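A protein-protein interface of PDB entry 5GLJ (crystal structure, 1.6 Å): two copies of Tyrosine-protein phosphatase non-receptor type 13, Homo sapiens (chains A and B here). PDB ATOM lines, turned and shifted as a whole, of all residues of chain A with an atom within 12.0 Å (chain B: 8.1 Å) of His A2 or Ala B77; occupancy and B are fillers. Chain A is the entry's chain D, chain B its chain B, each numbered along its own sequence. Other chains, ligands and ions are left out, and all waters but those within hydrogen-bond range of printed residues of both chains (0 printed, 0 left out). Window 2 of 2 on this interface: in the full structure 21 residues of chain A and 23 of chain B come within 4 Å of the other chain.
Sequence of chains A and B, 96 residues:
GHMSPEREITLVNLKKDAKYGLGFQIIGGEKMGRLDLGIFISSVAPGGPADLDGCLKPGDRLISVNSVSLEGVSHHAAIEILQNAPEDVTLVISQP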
ATOM      1  N   GLY A   1      13.208  26.228  34.016  1.00  0.00           N
ATOM      2  CA  GLY A   1      14.465  26.928  33.821  1.00  0.00           C
ATOM      3  C   GLY A   1      15.533  25.992  33.281  1.00  0.00           C
ATOM      4  O   GLY A   1      15.412  24.775  33.394  1.00  0.00           O
ATOM      5  N   HIS A   2      16.579  26.555  32.687  1.00  0.00           N
ATOM      6  CA  HIS A   2      17.640  25.735  32.106  1.00  0.00           C
ATOM      7  C   HIS A   2      18.919  26.530  31.893  1.00  0.00           C
ATOM      8  O   HIS A   2      18.907  27.764  31.903  1.00  0.00           O
ATOM      9  CB  HIS A   2      17.183  25.133  30.776  1.00  0.00           C
ATOM     10  CG  HIS A   2      16.887  26.152  29.716  1.00  0.00           C
ATOM     11  ND1 HIS A   2      15.622  26.658  29.504  1.00  0.00           N
ATOM     12  CD2 HIS A   2      17.693  26.755  28.808  1.00  0.00           C
ATOM     13  CE1 HIS A   2      15.660  27.527  28.507  1.00  0.00           C
ATOM     14  NE2 HIS A   2      16.904  27.603  28.066  1.00  0.00           N
ATOM     15  N   MET A   3      20.019  25.808  31.712  1.00  0.00           N
ATOM     16  CA  MET A   3      21.291  26.405  31.330  1.00  0.00           C
ATOM     17  C   MET A   3      21.137  27.037  29.955  1.00  0.00           C
ATOM     18  O   MET A   3      20.675  26.385  29.021  1.00  0.00           O
ATOM     19  CB  MET A   3      22.403  25.352  31.311  1.00  0.00           C
ATOM     20  CG  MET A   3      22.629  24.639  32.640  1.00  0.00           C
ATOM     21  SD  MET A   3      23.707  25.548  33.767  1.00  0.00           S
ATOM     22  CE  MET A   3      25.227  24.633  33.603  1.00  0.00           C
ATOM     23  N   SER A   4      21.508  28.305  29.836  1.00  0.00           N
ATOM     24  CA  SER A   4      21.425  29.009  28.562  1.00  0.00           C
ATOM     25  C   SER A   4      22.333  28.342  27.523  1.00  0.00           C
ATOM     26  O   SER A   4      23.502  28.076  27.809  1.00  0.00           O
ATOM     27  CB  SER A   4      21.802  30.480  28.756  1.00  0.00           C
ATOM     28  OG  SER A   4      21.718  31.198  27.538  1.00  0.00           O
ATOM     29  N   PRO A   5      21.792  28.044  26.323  1.00  0.00           N
ATOM     30  CA  PRO A   5      22.612  27.431  25.267  1.00  0.00           C
ATOM     31  C   PRO A   5      23.805  28.310  24.929  1.00  0.00           C
ATOM     32  O   PRO A   5      23.666  29.529  24.939  1.00  0.00           O
ATOM     33  CB  PRO A   5      21.654  27.335  24.073  1.00  0.00           C
ATOM     34  CG  PRO A   5      20.290  27.375  24.673  1.00  0.00           C
ATOM     35  CD  PRO A   5      20.403  28.263  25.883  1.00  0.00           C
ATOM     36  N   GLU A   6      24.946  27.710  24.625  1.00  0.00           N
ATOM     37  CA  GLU A   6      26.154  28.486  24.395  1.00  0.00           C
ATOM     38  C   GLU A   6      26.429  28.825  22.924  1.00  0.00           C
ATOM     39  O   GLU A   6      27.037  29.858  22.630  1.00  0.00           O
ATOM     40  CB  GLU A   6      27.348  27.736  24.966  1.00  0.00           C
ATOM     41  CG  GLU A   6      27.479  26.340  24.406  1.00  0.00           C
ATOM     42  CD  GLU A   6      28.915  25.927  24.222  1.00  0.00           C
ATOM     43  OE1 GLU A   6      29.255  24.793  24.607  1.00  0.00           O
ATOM     44  OE2 GLU A   6      29.710  26.735  23.688  1.00  0.00           O
ATOM     45  N   ARG A   7      25.997  27.967  22.004  1.00  0.00           N
ATOM     46  CA  ARG A   7      26.423  28.089  20.612  1.00  0.00           C
ATOM     47  C   ARG A   7      25.353  28.726  19.742  1.00  0.00           C
ATOM     48  O   ARG A   7      24.196  28.848  20.149  1.00  0.00           O
ATOM     49  CB  ARG A   7      26.809  26.713  20.055  1.00  0.00           C
ATOM     50  CG  ARG A   7      27.945  26.051  20.837  1.00  0.00           C
ATOM     51  CD  ARG A   7      28.303  24.664  20.323  1.00  0.00           C
ATOM     52  NE  ARG A   7      28.805  24.663  18.950  1.00  0.00           N
ATOM     53  CZ  ARG A   7      30.074  24.862  18.612  1.00  0.00           C
ATOM     54  NH1 ARG A   7      30.433  24.831  17.326  1.00  0.00           N
ATOM     55  NH2 ARG A   7      30.984  25.101  19.554  1.00  0.00           N
ATOM     56  N   ILE B  26       8.297  17.536  20.193  1.00  0.00           N
ATOM     57  CA  ILE B  26       9.661  17.053  20.073  1.00  0.00           C
ATOM     58  C   ILE B  26       9.946  15.914  21.042  1.00  0.00           C
ATOM     59  O   ILE B  26       9.266  15.755  22.063  1.00  0.00           O
ATOM     60  CB  ILE B  26      10.696  18.177  20.308  1.00  0.00           C
ATOM     61  CG1 ILE B  26      10.511  18.811  21.690  1.00  0.00           C
ATOM     62  CG2 ILE B  26      10.587  19.230  19.200  1.00  0.00           C
ATOM     63  CD1 ILE B  26      11.638  19.737  22.096  1.00  0.00           C
ATOM     64  N   GLY B  29      16.618  12.764  24.449  1.00  0.00           N
ATOM     65  CA  GLY B  29      17.101  12.456  25.787  1.00  0.00           C
ATOM     66  C   GLY B  29      17.378  13.707  26.600  1.00  0.00           C
ATOM     67  O   GLY B  29      17.175  14.819  26.113  1.00  0.00           O
ATOM     68  N   GLU B  30      17.840  13.525  27.836  1.00  0.00           N
ATOM     69  CA  GLU B  30      18.180  14.649  28.708  1.00  0.00           C
ATOM     70  C   GLU B  30      19.684  14.829  28.898  1.00  0.00           C
ATOM     71  O   GLU B  30      20.136  15.896  29.313  1.00  0.00           O
ATOM     72  CB  GLU B  30      17.528  14.482  30.079  1.00  0.00           C
ATOM     73  CG  GLU B  30      16.032  14.278  30.029  1.00  0.00           C
ATOM     74  CD  GLU B  30      15.288  15.481  29.474  1.00  0.00           C
ATOM     75  OE1 GLU B  30      14.137  15.292  29.043  1.00  0.00           O
ATOM     76  OE2 GLU B  30      15.843  16.606  29.483  1.00  0.00           O
ATOM     77  N   ILE B  39      17.609  16.477  19.515  1.00  0.00           N
ATOM     78  CA  ILE B  39      16.211  16.889  19.507  1.00  0.00           C
ATOM     79  C   ILE B  39      15.597  16.613  18.144  1.00  0.00           C
ATOM     80  O   ILE B  39      16.110  17.066  17.129  1.00  0.00           O
ATOM     81  CB  ILE B  39      16.049  18.390  19.850  1.00  0.00           C
ATOM     82  CG1 ILE B  39      16.758  18.717  21.172  1.00  0.00           C
ATOM     83  CG2 ILE B  39      14.561  18.783  19.896  1.00  0.00           C
ATOM     84  CD1 ILE B  39      16.199  17.972  22.358  1.00  0.00           C
ATOM     85  N   VAL B  68      19.739  30.269  17.823  1.00  0.00           N
ATOM     86  CA  VAL B  68      20.260  29.614  19.017  1.00  0.00           C
ATOM     87  C   VAL B  68      20.435  28.122  18.737  1.00  0.00           C
ATOM     88  O   VAL B  68      19.471  27.433  18.443  1.00  0.00           O
ATOM     89  CB  VAL B  68      19.348  29.825  20.227  1.00  0.00           C
ATOM     90  CG1 VAL B  68      19.892  29.063  21.430  1.00  0.00           C
ATOM     91  CG2 VAL B  68      19.247  31.309  20.540  1.00  0.00           C
ATOM     92  N   LEU B  70      20.904  24.151  19.236  1.00  0.00           N
ATOM     93  CA  LEU B  70      20.451  23.149  20.187  1.00  0.00           C
ATOM     94  C   LEU B  70      21.557  22.142  20.496  1.00  0.00           C
ATOM     95  O   LEU B  70      21.299  21.095  21.101  1.00  0.00           O
ATOM     96  CB  LEU B  70      19.218  22.427  19.655  1.00  0.00           C
ATOM     97  CG  LEU B  70      17.973  23.321  19.587  1.00  0.00           C
ATOM     98  CD1 LEU B  70      16.730  22.487  19.515  1.00  0.00           C
ATOM     99  CD2 LEU B  70      17.903  24.281  20.785  1.00  0.00           C
ATOM    100  N   GLY B  72      24.125  20.449  22.549  1.00  0.00           N
ATOM    101  CA  GLY B  72      24.264  20.296  23.985  1.00  0.00           C
ATOM    102  C   GLY B  72      23.004  20.601  24.766  1.00  0.00           C
ATOM    103  O   GLY B  72      23.045  20.704  25.989  1.00  0.00           O
ATOM    104  N   VAL B  73      21.881  20.749  24.074  1.00  0.00           N
ATOM    105  CA  VAL B  73      20.651  21.153  24.740  1.00  0.00           C
ATOM    106  C   VAL B  73      19.746  19.947  25.003  1.00  0.00           C
ATOM    107  O   VAL B  73      19.461  19.165  24.104  1.00  0.00           O
ATOM    108  CB  VAL B  73      19.902  22.230  23.919  1.00  0.00           C
ATOM    109  CG1 VAL B  73      18.588  22.602  24.586  1.00  0.00           C
ATOM    110  CG2 VAL B  73      20.805  23.474  23.739  1.00  0.00           C
ATOM    111  N   SER B  74      19.317  19.798  26.258  1.00  0.00           N
ATOM    112  CA  SER B  74      18.463  18.688  26.666  1.00  0.00           C
ATOM    113  C   SER B  74      17.040  18.831  26.143  1.00  0.00           C
ATOM    114  O   SER B  74      16.609  19.925  25.783  1.00  0.00           O
ATOM    115  CB  SER B  74      18.419  18.592  28.188  1.00  0.00           C
ATOM    116  OG  SER B  74      17.822  19.761  28.734  1.00  0.00           O
ATOM    117  N   HIS B  75      16.294  17.730  26.133  1.00  0.00           N
ATOM    118  CA  HIS B  75      14.883  17.786  25.771  1.00  0.00           C
ATOM    119  C   HIS B  75      14.139  18.816  26.624  1.00  0.00           C
ATOM    120  O   HIS B  75      13.369  19.620  26.107  1.00  0.00           O
ATOM    121  CB  HIS B  75      14.220  16.412  25.919  1.00  0.00           C
ATOM    122  CG  HIS B  75      12.784  16.391  25.485  1.00  0.00           C
ATOM    123  ND1 HIS B  75      11.747  16.719  26.329  1.00  0.00           N
ATOM    124  CD2 HIS B  75      12.216  16.075  24.298  1.00  0.00           C
ATOM    125  CE1 HIS B  75      10.599  16.620  25.677  1.00  0.00           C
ATOM    126  NE2 HIS B  75      10.857  16.223  24.444  1.00  0.00           N
ATOM    127  N   HIS B  76      14.392  18.802  27.933  1.00  0.00           N
ATOM    128  CA  HIS B  76      13.699  19.704  28.838  1.00  0.00           C
ATOM    129  C   HIS B  76      14.002  21.165  28.494  1.00  0.00           C
ATOM    130  O   HIS B  76      13.102  22.000  28.453  1.00  0.00           O
ATOM    131  CB  HIS B  76      14.086  19.406  30.290  1.00  0.00           C
ATOM    132  CG  HIS B  76      14.161  20.626  31.152  1.00  0.00           C
ATOM    133  ND1 HIS B  76      13.039  21.287  31.603  1.00  0.00           N
ATOM    134  CD2 HIS B  76      15.223  21.317  31.627  1.00  0.00           C
ATOM    135  CE1 HIS B  76      13.407  22.335  32.319  1.00  0.00           C
ATOM    136  NE2 HIS B  76      14.727  22.373  32.351  1.00  0.00           N
ATOM    137  N   ALA B  77      15.268  21.461  28.237  1.00  0.00           N
ATOM    138  CA  ALA B  77      15.675  22.812  27.893  1.00  0.00           C
ATOM    139  C   ALA B  77      15.117  23.222  26.527  1.00  0.00           C
ATOM    140  O   ALA B  77      14.753  24.376  26.329  1.00  0.00           O
ATOM    141  CB  ALA B  77      17.200  22.931  27.910  1.00  0.00           C
ATOM    142  N   ALA B  78      15.029  22.272  25.597  1.00  0.00           N
ATOM    143  CA  ALA B  78      14.504  22.576  24.266  1.00  0.00           C
ATOM    144  C   ALA B  78      13.012  22.902  24.301  1.00  0.00           C
ATOM    145  O   ALA B  78      12.548  23.778  23.573  1.00  0.00           O
ATOM    146  CB  ALA B  78      14.772  21.419  23.317  1.00  0.00           C
ATOM    147  N   ILE B  79      12.253  22.196  25.139  1.00  0.00           N
ATOM    148  CA  ILE B  79      10.834  22.513  25.291  1.00  0.00           C
ATOM    149  C   ILE B  79      10.649  23.944  25.788  1.00  0.00           C
ATOM    150  O   ILE B  79       9.818  24.696  25.278  1.00  0.00           O
ATOM    151  CB  ILE B  79      10.133  21.543  26.263  1.00  0.00           C
ATOM    152  CG1 ILE B  79      10.014  20.164  25.623  1.00  0.00           C
ATOM    153  CG2 ILE B  79       8.763  22.077  26.639  1.00  0.00           C
ATOM    154  CD1 ILE B  79       8.819  20.010  24.715  1.00  0.00           C
ATOM    155  N   GLU B  80      11.443  24.318  26.781  1.00  0.00           N
ATOM    156  CA  GLU B  80      11.389  25.673  27.309  1.00  0.00           C
ATOM    157  C   GLU B  80      11.795  26.712  26.257  1.00  0.00           C
ATOM    158  O   GLU B  80      11.137  27.747  26.126  1.00  0.00           O
ATOM    159  CB  GLU B  80      12.271  25.789  28.554  1.00  0.00           C
ATOM    160  CG  GLU B  80      11.724  25.011  29.731  1.00  0.00           C
ATOM    161  CD  GLU B  80      12.370  25.393  31.044  1.00  0.00           C
ATOM    162  OE1 GLU B  80      13.480  25.966  31.018  1.00  0.00           O
ATOM    163  OE2 GLU B  80      11.755  25.129  32.102  1.00  0.00           O
ATOM    164  N   ILE B  81      12.848  26.430  25.494  1.00  0.00           N
ATOM    165  CA  ILE B  81      13.250  27.322  24.405  1.00  0.00           C
ATOM    166  C   ILE B  81      12.104  27.529  23.409  1.00  0.00           C
ATOM    167  O   ILE B  81      11.822  28.659  23.005  1.00  0.00           O
ATOM    168  CB  ILE B  81      14.493  26.789  23.660  1.00  0.00           C
ATOM    169  CG1 ILE B  81      15.733  26.941  24.540  1.00  0.00           C
ATOM    170  CG2 ILE B  81      14.715  27.534  22.336  1.00  0.00           C
ATOM    171  CD1 ILE B  81      16.937  26.247  23.989  1.00  0.00           C
ATOM    172  N   LEU B  82      11.440  26.445  23.024  1.00  0.00           N
ATOM    173  CA  LEU B  82      10.335  26.540  22.063  1.00  0.00           C
ATOM    174  C   LEU B  82       9.124  27.255  22.670  1.00  0.00           C
ATOM    175  O   LEU B  82       8.520  28.104  22.020  1.00  0.00           O
ATOM    176  CB  LEU B  82       9.940  25.153  21.560  1.00  0.00           C
ATOM    177  CG  LEU B  82      11.004  24.449  20.712  1.00  0.00           C
ATOM    178  CD1 LEU B  82      10.674  22.986  20.529  1.00  0.00           C
ATOM    179  CD2 LEU B  82      11.181  25.135  19.357  1.00  0.00           C
ATOM    180  N   GLN B  83       8.789  26.932  23.918  1.00  0.00           N
ATOM    181  CA  GLN B  83       7.660  27.571  24.582  1.00  0.00           C
ATOM    182  C   GLN B  83       7.910  29.059  24.816  1.00  0.00           C
ATOM    183  O   GLN B  83       6.996  29.870  24.678  1.00  0.00           O
ATOM    184  CB  GLN B  83       7.347  26.873  25.905  1.00  0.00           C
ATOM    185  CG  GLN B  83       6.719  25.504  25.720  1.00  0.00           C
ATOM    186  CD  GLN B  83       6.267  24.877  27.023  1.00  0.00           C
ATOM    187  OE1 GLN B  83       6.490  25.425  28.105  1.00  0.00           O
ATOM    188  NE2 GLN B  83       5.615  23.723  26.926  1.00  0.00           N
ATOM    189  N   ASN B  84       9.152  29.406  25.153  1.00  0.00           N
ATOM    190  CA  ASN B  84       9.522  30.787  25.466  1.00  0.00           C
ATOM    191  C   ASN B  84       9.789  31.631  24.230  1.00  0.00           C
ATOM    192  O   ASN B  84       9.925  32.848  24.320  1.00  0.00           O
ATOM    193  CB  ASN B  84      10.762  30.826  26.373  1.00  0.00           C
ATOM    194  CG  ASN B  84      10.492  30.282  27.769  1.00  0.00           C
ATOM    195  OD1 ASN B  84       9.337  30.098  28.175  1.00  0.00           O
ATOM    196  ND2 ASN B  84      11.563  30.028  28.519  1.00  0.00           N
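Of the 19 printed residues of chain B, 6 touch a printed residue of chain A. Along chain B the printed residues that touch a printed residue of chain A span positions 68 to 81. Among the printed residues, 8 pairs touch across the chains.
No position is printed for both chains. Of the 8 pairs that touch across the chains among the printed residues, none has its exchanged pair printed and touching as well.
Among the printed residues, pairs that only touch across the chains: His A2 with Ala B77 (3.6 Å), His A2 with Ile B81 (3.8 Å), Pro A5 with Val B68 (3.6 Å), Pro A5 with Val B73 (3.97 Å) and Pro A5 with Ile B81 (3.6 Å).
Of the printed residues of chain B, His A2 touches Ala B77, Glu B80 and Ile B81. Ile B26 touches none of the printed residues of chain A. Ile B39 touches none of the printed residues of chain A. Of the printed residues of chain A, Val B68 touches Pro A5. No residue of chain A comes within 4 Å of Ser B74. No residue of chain A comes within 4 Å of His B75. Of the printed residues of chain A, His B76 touches Gly A1 (2.7 Å). Ala B77 touches just one residue of chain A: His A2 (3.6 Å). No residue of chain A comes within 4 Å of Ala B78. No residue of chain A comes within 4 Å of Ile B79. Of the printed residues of chain A, Ile B81 touches His A2 (3.8 Å) and Pro A5 (3.6 Å). The nearest printed residue of chain A that does not touch His B76 is His A2 (4.02 Å).
The backbone NH (N) of His B76 lies within hydrogen-bond range of the side-chain carboxylate (OE2) of Glu B30 (3.1 Å). OG of Ser B74 is in hydrogen-bond range of N of Ala B77, 3.1 Å away. ND2 of Asn B84 sits close to O of Glu B80 (3.3 Å).
NE2 of His B76 lies within hydrogen-bond range of O of Gly A1, at 2.7 Å. The side-chain carboxylate (OE2) of Glu B80 lies within hydrogen-bond range of the backbone NH (N) of Gly A1, 2.6 Å away. The side-chain carboxylate (OE1) of Glu B80 is in hydrogen-bond range of a ring nitrogen (ND1) of His A2 (2.7 Å).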
